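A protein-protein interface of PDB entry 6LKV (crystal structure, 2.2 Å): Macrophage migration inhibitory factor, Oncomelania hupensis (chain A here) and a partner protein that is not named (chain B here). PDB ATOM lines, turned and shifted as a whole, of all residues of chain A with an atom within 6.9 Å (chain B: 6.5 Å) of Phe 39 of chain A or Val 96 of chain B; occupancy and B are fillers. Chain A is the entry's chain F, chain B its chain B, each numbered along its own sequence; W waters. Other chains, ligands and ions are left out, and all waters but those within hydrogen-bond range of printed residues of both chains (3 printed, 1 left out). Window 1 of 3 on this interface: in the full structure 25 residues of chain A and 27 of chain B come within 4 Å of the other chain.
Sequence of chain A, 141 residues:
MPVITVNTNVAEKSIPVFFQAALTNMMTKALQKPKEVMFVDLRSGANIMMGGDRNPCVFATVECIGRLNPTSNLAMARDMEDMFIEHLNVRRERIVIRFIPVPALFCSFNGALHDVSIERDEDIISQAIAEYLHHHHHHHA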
ATOM      1  N   MET A   1      12.608 -31.139  10.609  1.00  0.00           N
ATOM      2  CA  MET A   1      12.428 -31.481  12.028  1.00  0.00           C
ATOM      3  C   MET A   1      13.029 -30.393  12.944  1.00  0.00           C
ATOM      4  O   MET A   1      13.925 -29.645  12.513  1.00  0.00           O
ATOM      5  CB  MET A   1      13.072 -32.845  12.271  1.00  0.00           C
ATOM      6  CG  MET A   1      14.470 -32.725  12.808  1.00  0.00           C
ATOM      7  SD  MET A   1      14.557 -32.433  14.617  1.00  0.00           S
ATOM      8  CE  MET A   1      16.149 -31.600  14.673  1.00  0.00           C
ATOM      9  N   PRO A   2      12.534 -30.222  14.218  1.00  0.00           N
ATOM     10  CA  PRO A   2      11.292 -30.818  14.673  1.00  0.00           C
ATOM     11  C   PRO A   2      10.203 -29.975  13.999  1.00  0.00           C
ATOM     12  O   PRO A   2      10.322 -28.766  13.893  1.00  0.00           O
ATOM     13  CB  PRO A   2      11.317 -30.785  16.203  1.00  0.00           C
ATOM     14  CG  PRO A   2      12.639 -30.135  16.553  1.00  0.00           C
ATOM     15  CD  PRO A   2      13.133 -29.449  15.296  1.00  0.00           C
ATOM     16  N   VAL A   3       9.252 -30.676  13.401  1.00  0.00           N
ATOM     17  CA  VAL A   3       8.072 -30.052  12.763  1.00  0.00           C
ATOM     18  C   VAL A   3       6.865 -30.695  13.411  1.00  0.00           C
ATOM     19  O   VAL A   3       6.757 -31.927  13.343  1.00  0.00           O
ATOM     20  CB  VAL A   3       8.090 -30.261  11.252  1.00  0.00           C
ATOM     21  CG1 VAL A   3       6.872 -29.633  10.596  1.00  0.00           C
ATOM     22  CG2 VAL A   3       9.402 -29.804  10.658  1.00  0.00           C
ATOM     23  N   ILE A   4       6.031 -29.855  14.017  1.00  0.00           N
ATOM     24  CA  ILE A   4       4.698 -30.228  14.547  1.00  0.00           C
ATOM     25  C   ILE A   4       3.688 -29.748  13.511  1.00  0.00           C
ATOM     26  O   ILE A   4       3.621 -28.505  13.264  1.00  0.00           O
ATOM     27  CB  ILE A   4       4.441 -29.589  15.916  1.00  0.00           C
ATOM     28  CG1 ILE A   4       5.696 -29.524  16.796  1.00  0.00           C
ATOM     29  CG2 ILE A   4       3.274 -30.276  16.612  1.00  0.00           C
ATOM     30  CD1 ILE A   4       6.324 -30.866  17.104  1.00  0.00           C
ATOM     31  N   THR A   5       2.942 -30.668  12.909  1.00  0.00           N
ATOM     32  CA  THR A   5       1.875 -30.338  11.933  1.00  0.00           C
ATOM     33  C   THR A   5       0.545 -30.627  12.615  1.00  0.00           C
ATOM     34  O   THR A   5       0.356 -31.763  13.105  1.00  0.00           O
ATOM     35  CB  THR A   5       2.075 -31.086  10.610  1.00  0.00           C
ATOM     36  OG1 THR A   5       3.409 -30.849  10.160  1.00  0.00           O
ATOM     37  CG2 THR A   5       1.127 -30.636   9.530  1.00  0.00           C
ATOM     38  N   THR A  24       4.893 -24.593  20.388  1.00  0.00           N
ATOM     39  CA  THR A  24       6.342 -24.410  20.171  1.00  0.00           C
ATOM     40  C   THR A  24       7.073 -24.569  21.517  1.00  0.00           C
ATOM     41  O   THR A  24       7.975 -25.426  21.613  1.00  0.00           O
ATOM     42  CB  THR A  24       6.657 -23.047  19.550  1.00  0.00           C
ATOM     43  OG1 THR A  24       6.074 -22.913  18.253  1.00  0.00           O
ATOM     44  CG2 THR A  24       8.149 -22.827  19.419  1.00  0.00           C
ATOM     45  N   LYS A  35      14.835 -24.099  20.296  1.00  0.00           N
ATOM     46  CA  LYS A  35      13.565 -23.443  19.905  1.00  0.00           C
ATOM     47  C   LYS A  35      13.654 -22.974  18.448  1.00  0.00           C
ATOM     48  O   LYS A  35      12.642 -23.079  17.745  1.00  0.00           O
ATOM     49  CB  LYS A  35      13.232 -22.288  20.852  1.00  0.00           C
ATOM     50  CG  LYS A  35      11.872 -21.662  20.587  1.00  0.00           C
ATOM     51  CD  LYS A  35      11.379 -20.714  21.642  1.00  0.00           C
ATOM     52  CE  LYS A  35      10.315 -19.794  21.092  1.00  0.00           C
ATOM     53  NZ  LYS A  35       9.472 -19.218  22.166  1.00  0.00           N
ATOM     54  N   GLU A  36      14.841 -22.528  18.021  1.00  0.00           N
ATOM     55  CA  GLU A  36      15.133 -21.900  16.707  1.00  0.00           C
ATOM     56  C   GLU A  36      14.614 -22.767  15.555  1.00  0.00           C
ATOM     57  O   GLU A  36      14.236 -22.200  14.530  1.00  0.00           O
ATOM     58  CB  GLU A  36      16.645 -21.690  16.541  1.00  0.00           C
ATOM     59  CG  GLU A  36      17.212 -20.531  17.350  1.00  0.00           C
ATOM     60  CD  GLU A  36      17.274 -20.669  18.872  1.00  0.00           C
ATOM     61  OE1 GLU A  36      17.302 -21.813  19.379  1.00  0.00           O
ATOM     62  OE2 GLU A  36      17.267 -19.613  19.554  1.00  0.00           O
ATOM     63  N   VAL A  37      14.685 -24.093  15.686  1.00  0.00           N
ATOM     64  CA  VAL A  37      14.399 -25.052  14.584  1.00  0.00           C
ATOM     65  C   VAL A  37      13.060 -25.755  14.854  1.00  0.00           C
ATOM     66  O   VAL A  37      12.770 -26.714  14.157  1.00  0.00           O
ATOM     67  CB  VAL A  37      15.557 -26.049  14.383  1.00  0.00           C
ATOM     68  CG1 VAL A  37      16.833 -25.327  14.022  1.00  0.00           C
ATOM     69  CG2 VAL A  37      15.786 -26.950  15.583  1.00  0.00           C
ATOM     70  N   MET A  38      12.268 -25.302  15.827  1.00  0.00           N
ATOM     71  CA  MET A  38      10.919 -25.873  16.057  1.00  0.00           C
ATOM     72  C   MET A  38       9.937 -25.191  15.099  1.00  0.00           C
ATOM     73  O   MET A  38       9.679 -23.981  15.255  1.00  0.00           O
ATOM     74  CB  MET A  38      10.471 -25.675  17.502  1.00  0.00           C
ATOM     75  CG  MET A  38       9.135 -26.338  17.828  1.00  0.00           C
ATOM     76  SD  MET A  38       9.180 -28.129  17.989  1.00  0.00           S
ATOM     77  CE  MET A  38      10.728 -28.338  18.875  1.00  0.00           C
ATOM     78  N   PHE A  39       9.399 -25.951  14.158  1.00  0.00           N
ATOM     79  CA  PHE A  39       8.297 -25.494  13.276  1.00  0.00           C
ATOM     80  C   PHE A  39       6.975 -25.948  13.863  1.00  0.00           C
ATOM     81  O   PHE A  39       6.899 -27.110  14.308  1.00  0.00           O
ATOM     82  CB  PHE A  39       8.377 -26.132  11.899  1.00  0.00           C
ATOM     83  CG  PHE A  39       9.490 -25.640  11.028  1.00  0.00           C
ATOM     84  CD1 PHE A  39      10.762 -26.185  11.127  1.00  0.00           C
ATOM     85  CD2 PHE A  39       9.242 -24.689  10.061  1.00  0.00           C
ATOM     86  CE1 PHE A  39      11.766 -25.763  10.282  1.00  0.00           C
ATOM     87  CE2 PHE A  39      10.255 -24.256   9.226  1.00  0.00           C
ATOM     88  CZ  PHE A  39      11.511 -24.805   9.330  1.00  0.00           C
ATOM     89  N   VAL A  40       5.970 -25.073  13.826  1.00  0.00           N
ATOM     90  CA  VAL A  40       4.551 -25.466  14.019  1.00  0.00           C
ATOM     91  C   VAL A  40       3.758 -24.996  12.801  1.00  0.00           C
ATOM     92  O   VAL A  40       3.669 -23.772  12.540  1.00  0.00           O
ATOM     93  CB  VAL A  40       3.960 -24.941  15.331  1.00  0.00           C
ATOM     94  CG1 VAL A  40       2.531 -25.437  15.501  1.00  0.00           C
ATOM     95  CG2 VAL A  40       4.821 -25.334  16.524  1.00  0.00           C
ATOM     96  N   ASP A  41       3.264 -25.976  12.041  1.00  0.00           N
ATOM     97  CA  ASP A  41       2.470 -25.772  10.811  1.00  0.00           C
ATOM     98  C   ASP A  41       1.016 -26.083  11.157  1.00  0.00           C
ATOM     99  O   ASP A  41       0.691 -27.249  11.331  1.00  0.00           O
ATOM    100  CB  ASP A  41       3.019 -26.640   9.687  1.00  0.00           C
ATOM    101  CG  ASP A  41       2.374 -26.406   8.336  1.00  0.00           C
ATOM    102  OD1 ASP A  41       1.437 -25.581   8.236  1.00  0.00           O
ATOM    103  OD2 ASP A  41       2.819 -27.071   7.403  1.00  0.00           O
ATOM    104  N   CYS A 107      17.856 -35.039   6.464  1.00  0.00           N
ATOM    105  CA  CYS A 107      17.274 -33.758   6.905  1.00  0.00           C
ATOM    106  C   CYS A 107      18.355 -32.674   6.962  1.00  0.00           C
ATOM    107  O   CYS A 107      19.335 -32.824   7.747  1.00  0.00           O
ATOM    108  CB  CYS A 107      16.593 -33.912   8.256  1.00  0.00           C
ATOM    109  SG  CYS A 107      15.653 -32.444   8.738  1.00  0.00           S
ATOM    110  N   SER A 108      18.154 -31.596   6.205  1.00  0.00           N
ATOM    111  CA  SER A 108      19.004 -30.379   6.173  1.00  0.00           C
ATOM    112  C   SER A 108      18.426 -29.267   7.055  1.00  0.00           C
ATOM    113  O   SER A 108      17.177 -29.136   7.177  1.00  0.00           O
ATOM    114  CB  SER A 108      19.199 -29.901   4.788  1.00  0.00           C
ATOM    115  OG  SER A 108      17.955 -29.590   4.151  1.00  0.00           O
ATOM    116  N   PHE A 109      19.317 -28.511   7.696  1.00  0.00           N
ATOM    117  CA  PHE A 109      19.048 -27.184   8.284  1.00  0.00           C
ATOM    118  C   PHE A 109      20.241 -26.282   7.956  1.00  0.00           C
ATOM    119  O   PHE A 109      21.398 -26.677   8.206  1.00  0.00           O
ATOM    120  CB  PHE A 109      18.835 -27.285   9.790  1.00  0.00           C
ATOM    121  CG  PHE A 109      18.904 -25.948  10.478  1.00  0.00           C
ATOM    122  CD1 PHE A 109      18.032 -24.933  10.109  1.00  0.00           C
ATOM    123  CD2 PHE A 109      19.879 -25.672  11.442  1.00  0.00           C
ATOM    124  CE1 PHE A 109      18.088 -23.694  10.727  1.00  0.00           C
ATOM    125  CE2 PHE A 109      19.938 -24.423  12.046  1.00  0.00           C
ATOM    126  CZ  PHE A 109      19.036 -23.443  11.698  1.00  0.00           C
ATOM    127  N   ASN A 110      19.970 -25.125   7.367  1.00  0.00           N
ATOM    128  CA  ASN A 110      20.956 -24.026   7.225  1.00  0.00           C
ATOM    129  C   ASN A 110      22.202 -24.542   6.505  1.00  0.00           C
ATOM    130  O   ASN A 110      23.293 -24.266   6.982  1.00  0.00           O
ATOM    131  CB  ASN A 110      21.308 -23.458   8.595  1.00  0.00           C
ATOM    132  CG  ASN A 110      21.961 -22.095   8.577  1.00  0.00           C
ATOM    133  OD1 ASN A 110      21.957 -21.379   7.582  1.00  0.00           O
ATOM    134  ND2 ASN A 110      22.418 -21.680   9.744  1.00  0.00           N
ATOM    135  N   HIS A 114      22.394 -33.209   9.618  1.00  0.00           N
ATOM    136  CA  HIS A 114      22.468 -33.285  11.100  1.00  0.00           C
ATOM    137  C   HIS A 114      23.451 -34.386  11.488  1.00  0.00           C
ATOM    138  O   HIS A 114      23.697 -35.289  10.660  1.00  0.00           O
ATOM    139  CB  HIS A 114      21.067 -33.493  11.677  1.00  0.00           C
ATOM    140  CG  HIS A 114      20.151 -32.330  11.492  1.00  0.00           C
ATOM    141  ND1 HIS A 114      19.549 -32.038  10.274  1.00  0.00           N
ATOM    142  CD2 HIS A 114      19.713 -31.396  12.367  1.00  0.00           C
ATOM    143  CE1 HIS A 114      18.777 -30.978  10.424  1.00  0.00           C
ATOM    144  NE2 HIS A 114      18.861 -30.559  11.690  1.00  0.00           N
ATOM    145  N   ASN B   7       6.308 -25.996   2.187  1.00  0.00           N
ATOM    146  CA  ASN B   7       5.443 -25.375   3.203  1.00  0.00           C
ATOM    147  C   ASN B   7       6.108 -24.057   3.586  1.00  0.00           C
ATOM    148  O   ASN B   7       7.212 -24.121   4.168  1.00  0.00           O
ATOM    149  CB  ASN B   7       5.266 -26.259   4.427  1.00  0.00           C
ATOM    150  CG  ASN B   7       4.685 -27.607   4.080  1.00  0.00           C
ATOM    151  OD1 ASN B   7       3.478 -27.684   3.828  1.00  0.00           O
ATOM    152  ND2 ASN B   7       5.538 -28.641   4.034  1.00  0.00           N
ATOM    153  N   ILE B  48       2.588 -21.326   9.053  1.00  0.00           N
ATOM    154  CA  ILE B  48       3.772 -22.046   9.558  1.00  0.00           C
ATOM    155  C   ILE B  48       4.702 -21.003  10.184  1.00  0.00           C
ATOM    156  O   ILE B  48       5.024 -19.998   9.539  1.00  0.00           O
ATOM    157  CB  ILE B  48       4.416 -22.893   8.444  1.00  0.00           C
ATOM    158  CG1 ILE B  48       5.521 -23.769   9.041  1.00  0.00           C
ATOM    159  CG2 ILE B  48       4.897 -22.044   7.285  1.00  0.00           C
ATOM    160  CD1 ILE B  48       5.994 -24.873   8.144  1.00  0.00           C
ATOM    161  N   MET B  49       5.063 -21.219  11.435  1.00  0.00           N
ATOM    162  CA  MET B  49       6.088 -20.413  12.146  1.00  0.00           C
ATOM    163  C   MET B  49       7.279 -21.320  12.480  1.00  0.00           C
ATOM    164  O   MET B  49       7.138 -22.568  12.441  1.00  0.00           O
ATOM    165  CB  MET B  49       5.497 -19.791  13.424  1.00  0.00           C
ATOM    166  CG  MET B  49       5.057 -20.766  14.474  1.00  0.00           C
ATOM    167  SD  MET B  49       4.794 -20.040  16.147  1.00  0.00           S
ATOM    168  CE  MET B  49       3.662 -18.722  15.707  1.00  0.00           C
ATOM    169  N   MET B  50       8.426 -20.716  12.755  1.00  0.00           N
ATOM    170  CA  MET B  50       9.680 -21.417  13.078  1.00  0.00           C
ATOM    171  C   MET B  50      10.359 -20.662  14.228  1.00  0.00           C
ATOM    172  O   MET B  50      10.475 -19.427  14.131  1.00  0.00           O
ATOM    173  CB  MET B  50      10.562 -21.440  11.833  1.00  0.00           C
ATOM    174  CG  MET B  50      11.857 -22.190  11.996  1.00  0.00           C
ATOM    175  SD  MET B  50      12.964 -21.863  10.630  1.00  0.00           S
ATOM    176  CE  MET B  50      14.355 -22.884  11.088  1.00  0.00           C
ATOM    177  N   GLY B  51      10.805 -21.359  15.271  1.00  0.00           N
ATOM    178  CA  GLY B  51      11.388 -20.706  16.460  1.00  0.00           C
ATOM    179  C   GLY B  51      10.395 -19.797  17.184  1.00  0.00           C
ATOM    180  O   GLY B  51      10.857 -18.860  17.863  1.00  0.00           O
ATOM    181  N   CYS B  57      10.023 -18.497   6.415  1.00  0.00           N
ATOM    182  CA  CYS B  57      10.616 -19.840   6.637  1.00  0.00           C
ATOM    183  C   CYS B  57      10.094 -20.830   5.590  1.00  0.00           C
ATOM    184  O   CYS B  57       9.058 -20.539   4.903  1.00  0.00           O
ATOM    185  CB  CYS B  57      10.356 -20.320   8.061  1.00  0.00           C
ATOM    186  SG  CYS B  57       8.617 -20.708   8.431  1.00  0.00           S
ATOM    187  N   VAL B  58      10.794 -21.961   5.447  1.00  0.00           N
ATOM    188  CA  VAL B  58      10.371 -23.085   4.572  1.00  0.00           C
ATOM    189  C   VAL B  58      10.609 -24.379   5.324  1.00  0.00           C
ATOM    190  O   VAL B  58      11.753 -24.585   5.789  1.00  0.00           O
ATOM    191  CB  VAL B  58      11.135 -23.119   3.241  1.00  0.00           C
ATOM    192  CG1 VAL B  58      10.717 -24.306   2.386  1.00  0.00           C
ATOM    193  CG2 VAL B  58      10.990 -21.825   2.458  1.00  0.00           C
ATOM    194  N   PHE B  59       9.582 -25.218   5.431  1.00  0.00           N
ATOM    195  CA  PHE B  59       9.759 -26.674   5.675  1.00  0.00           C
ATOM    196  C   PHE B  59       9.357 -27.399   4.395  1.00  0.00           C
ATOM    197  O   PHE B  59       8.206 -27.252   3.953  1.00  0.00           O
ATOM    198  CB  PHE B  59       9.014 -27.171   6.906  1.00  0.00           C
ATOM    199  CG  PHE B  59       9.102 -28.672   7.044  1.00  0.00           C
ATOM    200  CD1 PHE B  59      10.345 -29.298   7.092  1.00  0.00           C
ATOM    201  CD2 PHE B  59       7.960 -29.467   7.072  1.00  0.00           C
ATOM    202  CE1 PHE B  59      10.435 -30.681   7.220  1.00  0.00           C
ATOM    203  CE2 PHE B  59       8.063 -30.849   7.146  1.00  0.00           C
ATOM    204  CZ  PHE B  59       9.304 -31.450   7.204  1.00  0.00           C
ATOM    205  N   ALA B  60      10.310 -28.087   3.758  1.00  0.00           N
ATOM    206  CA  ALA B  60      10.045 -28.821   2.499  1.00  0.00           C
ATOM    207  C   ALA B  60      10.325 -30.315   2.685  1.00  0.00           C
ATOM    208  O   ALA B  60      11.170 -30.667   3.500  1.00  0.00           O
ATOM    209  CB  ALA B  60      10.858 -28.224   1.341  1.00  0.00           C
ATOM    210  N   THR B  61       9.673 -31.154   1.888  1.00  0.00           N
ATOM    211  CA  THR B  61       9.878 -32.611   1.869  1.00  0.00           C
ATOM    212  C   THR B  61      10.123 -33.050   0.434  1.00  0.00           C
ATOM    213  O   THR B  61       9.534 -32.454  -0.514  1.00  0.00           O
ATOM    214  CB  THR B  61       8.708 -33.355   2.532  1.00  0.00           C
ATOM    215  OG1 THR B  61       7.521 -33.152   1.768  1.00  0.00           O
ATOM    216  CG2 THR B  61       8.481 -32.917   3.957  1.00  0.00           C
ATOM    217  N   GLU B  81      17.722 -24.973  -1.171  1.00  0.00           N
ATOM    218  CA  GLU B  81      17.963 -23.759  -0.358  1.00  0.00           C
ATOM    219  C   GLU B  81      18.221 -22.563  -1.276  1.00  0.00           C
ATOM    220  O   GLU B  81      17.523 -21.525  -1.119  1.00  0.00           O
ATOM    221  CB  GLU B  81      19.150 -23.966   0.575  1.00  0.00           C
ATOM    222  CG  GLU B  81      18.796 -24.702   1.846  1.00  0.00           C
ATOM    223  CD  GLU B  81      20.018 -25.060   2.659  1.00  0.00           C
ATOM    224  OE1 GLU B  81      21.128 -24.789   2.149  1.00  0.00           O
ATOM    225  OE2 GLU B  81      19.864 -25.574   3.781  1.00  0.00           O
ATOM    226  N   PHE B  84      15.143 -21.404  -2.891  1.00  0.00           N
ATOM    227  CA  PHE B  84      14.221 -20.773  -1.916  1.00  0.00           C
ATOM    228  C   PHE B  84      14.743 -19.363  -1.571  1.00  0.00           C
ATOM    229  O   PHE B  84      13.930 -18.420  -1.448  1.00  0.00           O
ATOM    230  CB  PHE B  84      14.048 -21.657  -0.677  1.00  0.00           C
ATOM    231  CG  PHE B  84      13.459 -23.028  -0.902  1.00  0.00           C
ATOM    232  CD1 PHE B  84      12.682 -23.326  -2.015  1.00  0.00           C
ATOM    233  CD2 PHE B  84      13.633 -24.015   0.062  1.00  0.00           C
ATOM    234  CE1 PHE B  84      12.129 -24.597  -2.174  1.00  0.00           C
ATOM    235  CE2 PHE B  84      13.104 -25.290  -0.107  1.00  0.00           C
ATOM    236  CZ  PHE B  84      12.337 -25.577  -1.211  1.00  0.00           C
ATOM    237  N   ARG B  92      18.795 -18.886   4.530  1.00  0.00           N
ATOM    238  CA  ARG B  92      19.217 -20.307   4.631  1.00  0.00           C
ATOM    239  C   ARG B  92      18.935 -20.835   6.036  1.00  0.00           C
ATOM    240  O   ARG B  92      18.514 -22.002   6.136  1.00  0.00           O
ATOM    241  CB  ARG B  92      20.701 -20.475   4.297  1.00  0.00           C
ATOM    242  CG  ARG B  92      21.036 -21.867   3.796  1.00  0.00           C
ATOM    243  CD  ARG B  92      22.505 -22.071   3.530  1.00  0.00           C
ATOM    244  NE  ARG B  92      22.925 -21.289   2.382  1.00  0.00           N
ATOM    245  CZ  ARG B  92      22.822 -21.666   1.114  1.00  0.00           C
ATOM    246  NH1 ARG B  92      22.288 -22.839   0.793  1.00  0.00           N
ATOM    247  NH2 ARG B  92      23.243 -20.859   0.148  1.00  0.00           N
ATOM    248  N   ARG B  94      16.502 -20.312   7.848  1.00  0.00           N
ATOM    249  CA  ARG B  94      15.045 -20.497   8.074  1.00  0.00           C
ATOM    250  C   ARG B  94      14.508 -21.610   7.163  1.00  0.00           C
ATOM    251  O   ARG B  94      13.285 -21.629   6.887  1.00  0.00           O
ATOM    252  CB  ARG B  94      14.349 -19.161   7.851  1.00  0.00           C
ATOM    253  CG  ARG B  94      14.778 -18.065   8.817  1.00  0.00           C
ATOM    254  CD  ARG B  94      14.132 -18.232  10.166  1.00  0.00           C
ATOM    255  NE  ARG B  94      12.698 -17.996  10.102  1.00  0.00           N
ATOM    256  CZ  ARG B  94      11.880 -18.094  11.142  1.00  0.00           C
ATOM    257  NH1 ARG B  94      12.344 -18.447  12.332  1.00  0.00           N
ATOM    258  NH2 ARG B  94      10.593 -17.857  10.990  1.00  0.00           N
ATOM    259  N   ILE B  95      15.386 -22.517   6.706  1.00  0.00           N
ATOM    260  CA  ILE B  95      15.016 -23.616   5.777  1.00  0.00           C
ATOM    261  C   ILE B  95      15.422 -24.973   6.365  1.00  0.00           C
ATOM    262  O   ILE B  95      16.625 -25.160   6.733  1.00  0.00           O
ATOM    263  CB  ILE B  95      15.644 -23.417   4.394  1.00  0.00           C
ATOM    264  CG1 ILE B  95      15.255 -22.067   3.795  1.00  0.00           C
ATOM    265  CG2 ILE B  95      15.283 -24.569   3.467  1.00  0.00           C
ATOM    266  CD1 ILE B  95      16.033 -21.707   2.552  1.00  0.00           C
ATOM    267  N   VAL B  96      14.452 -25.882   6.445  1.00  0.00           N
ATOM    268  CA  VAL B  96      14.656 -27.309   6.780  1.00  0.00           C
ATOM    269  C   VAL B  96      13.991 -28.122   5.681  1.00  0.00           C
ATOM    270  O   VAL B  96      12.853 -27.777   5.265  1.00  0.00           O
ATOM    271  CB  VAL B  96      14.092 -27.648   8.169  1.00  0.00           C
ATOM    272  CG1 VAL B  96      13.976 -29.149   8.400  1.00  0.00           C
ATOM    273  CG2 VAL B  96      14.911 -26.982   9.273  1.00  0.00           C
ATOM    274  N   ILE B  97      14.714 -29.119   5.166  1.00  0.00           N
ATOM    275  CA  ILE B  97      14.196 -30.076   4.152  1.00  0.00           C
ATOM    276  C   ILE B  97      14.310 -31.492   4.719  1.00  0.00           C
ATOM    277  O   ILE B  97      15.346 -31.829   5.287  1.00  0.00           O
ATOM    278  CB  ILE B  97      14.961 -29.910   2.843  1.00  0.00           C
ATOM    279  CG1 ILE B  97      15.009 -28.443   2.390  1.00  0.00           C
ATOM    280  CG2 ILE B  97      14.393 -30.826   1.786  1.00  0.00           C
ATOM    281  CD1 ILE B  97      16.005 -28.191   1.298  1.00  0.00           C
ATOM    282  N   ARG B  98      13.260 -32.281   4.569  1.00  0.00           N
ATOM    283  CA  ARG B  98      13.250 -33.712   4.920  1.00  0.00           C
ATOM    284  C   ARG B  98      13.195 -34.531   3.632  1.00  0.00           C
ATOM    285  O   ARG B  98      12.339 -34.276   2.798  1.00  0.00           O
ATOM    286  CB  ARG B  98      12.094 -34.034   5.863  1.00  0.00           C
ATOM    287  CG  ARG B  98      12.057 -35.496   6.266  1.00  0.00           C
ATOM    288  CD  ARG B  98      10.798 -35.813   7.048  1.00  0.00           C
ATOM    289  NE  ARG B  98      10.656 -37.250   7.002  1.00  0.00           N
ATOM    290  CZ  ARG B  98       9.527 -37.913   7.077  1.00  0.00           C
ATOM    291  NH1 ARG B  98       8.375 -37.285   7.266  1.00  0.00           N
ATOM    292  NH2 ARG B  98       9.571 -39.223   6.961  1.00  0.00           N
HETATM  293  O   HOH W   1      14.813 -19.688  13.617  1.00  0.00           O
HETATM  294  O   HOH W   2       7.513 -22.381  16.107  1.00  0.00           O
HETATM  295  O   HOH W   3      17.555 -26.903   4.772  1.00  0.00           O
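Of the printed residues of chain B, Phe 39 of chain A touches Ile 48 (3.8 Å), Met 49 (3.3 Å), Met 50 (3.5 Å), Cys 57 (3.99 Å), Val 58 (3.6 Å), Phe 59 (3.9 Å) and Val 96 (3.5 Å).
His 114 of chain A touches none of the printed residues of chain B.
Of the printed residues of chain A, Gly 51 of chain B touches Lys 35, Glu 36 and Met 38.
Printed residues of chain A within 4 Å of Val 58 of chain B: Phe 39.
Arg 94 of chain B touches none of the printed residues of chain A.
Val 96 of chain B touches five residues of chain A.
The nearest printed residue of chain B that does not touch Phe 39 of chain A is Arg 94 of chain B (4.4 Å).
The nearest printed residue of chain B that does not touch Met 38 of chain A is Met 49 of chain B (4.05 Å).
The backbone carbonyl oxygen (O) of Met 50 of chain B is in hydrogen-bond range of the guanidinium group (NH1) of Arg 94 of chain B (2.8 Å).
The backbone NH (N) of Asn 7 of chain B is in hydrogen-bond range of the backbone carbonyl oxygen (O) of Phe 59 of chain B (2.9 Å).
The backbone carbonyl oxygen of Phe 39 of chain A sits at hydrogen-bond distance from the backbone NH of Ile 4 of chain A, 2.9 Å away.
The backbone carbonyl oxygen (O) of Cys 107 of chain A lies within hydrogen-bond range of a ring nitrogen (ND1) of His 114 of chain A (2.7 Å).
O of Ile 4 of chain A sits at hydrogen-bond distance from N of Asp 41 of chain A, 2.8 Å away.
CG1 of Val 96 of chain B touches N of Met 1 of chain A, at 3.3 Å.
Glu 36 of chain A touches Met 50 of chain B.
Gly 51 of chain B touches Glu 36 of chain A (N to O, 3.6 Å).
CE2 of Phe 39 of chain A touches SG of Cys 57 of chain B, 3.99 Å away.
Val 58 of chain B touches Phe 39 of chain A.
CB of Phe 59 of chain B touches CE2 of Phe 39 of chain A, 3.9 Å away.
CG2 of Val 96 of chain B touches CE1 of Phe 39 of chain A (3.5 Å).
Asp 41 of chain A touches Asn 7 of chain B.
Ile 48 of chain B touches Asp 41 of chain A.
Arg 92 of chain B touches Asn 110 of chain A.
The backbone carbonyl oxygen of Met 38 of chain A sits at hydrogen-bond distance from the backbone NH of Gly 51 of chain B, at 2.9 Å.
The backbone carbonyl oxygen (O) of Met 49 of chain B is in hydrogen-bond range of the backbone NH (N) of Val 40 of chain A, at 3.1 Å.
The side-chain hydroxyl (OG1) of Thr 24 of chain A lies within hydrogen-bond range of the side-chain sulfur (SD) of Met 49 of chain B, at 3.8 Å.
The backbone NH of Asn 110 of chain A is in hydrogen-bond range of the backbone carbonyl oxygen of Ile 95 of chain B (3.4 Å).
The side-chain sulfur (SG) of Cys 107 of chain A sits close to the backbone carbonyl oxygen (O) of Ile 97 of chain B, at 3.5 Å.
O of Ile 97 of chain B sits at hydrogen-bond distance from N of Ser 108 of chain A, at 3.0 Å.
Water W2 lies within hydrogen-bond range of OG1 of Thr 24 of chain A (2.6 Å), O of Met 38 of chain A (2.8 Å) and SD of Met 49 of chain B (3.6 Å).
Water W1 bridges O of Glu 36 of chain A (2.7 Å) and NH1 of Arg 94 of chain B (3.0 Å).
Water W3 lies within hydrogen-bond range of O of Ile 95 of chain B (2.8 Å), OG of Ser 108 of chain A (2.8 Å) and OE2 of Glu 81 of chain B (2.8 Å).
Printed residues of chain A that touch a printed residue of chain B: Met 1, Val 3, Thr 24, Lys 35, Glu 36, Met 38, Phe 39, Val 40, Asp 41, Cys 107, Ser 108, Phe 109 and Asn 110.
Hydrophobic or aromatic side chains of chain A within 4 Å of the printed part of chain B: Val 3, Phe 39 and Phe 109.
Hydrophobic or aromatic side chains of chain B within 4 Å of the printed part of chain A: Ile 48, Met 49, Met 50, Phe 59, Val 96 and Ile 97.
Among the printed residues, 29 pairs touch across the chains.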
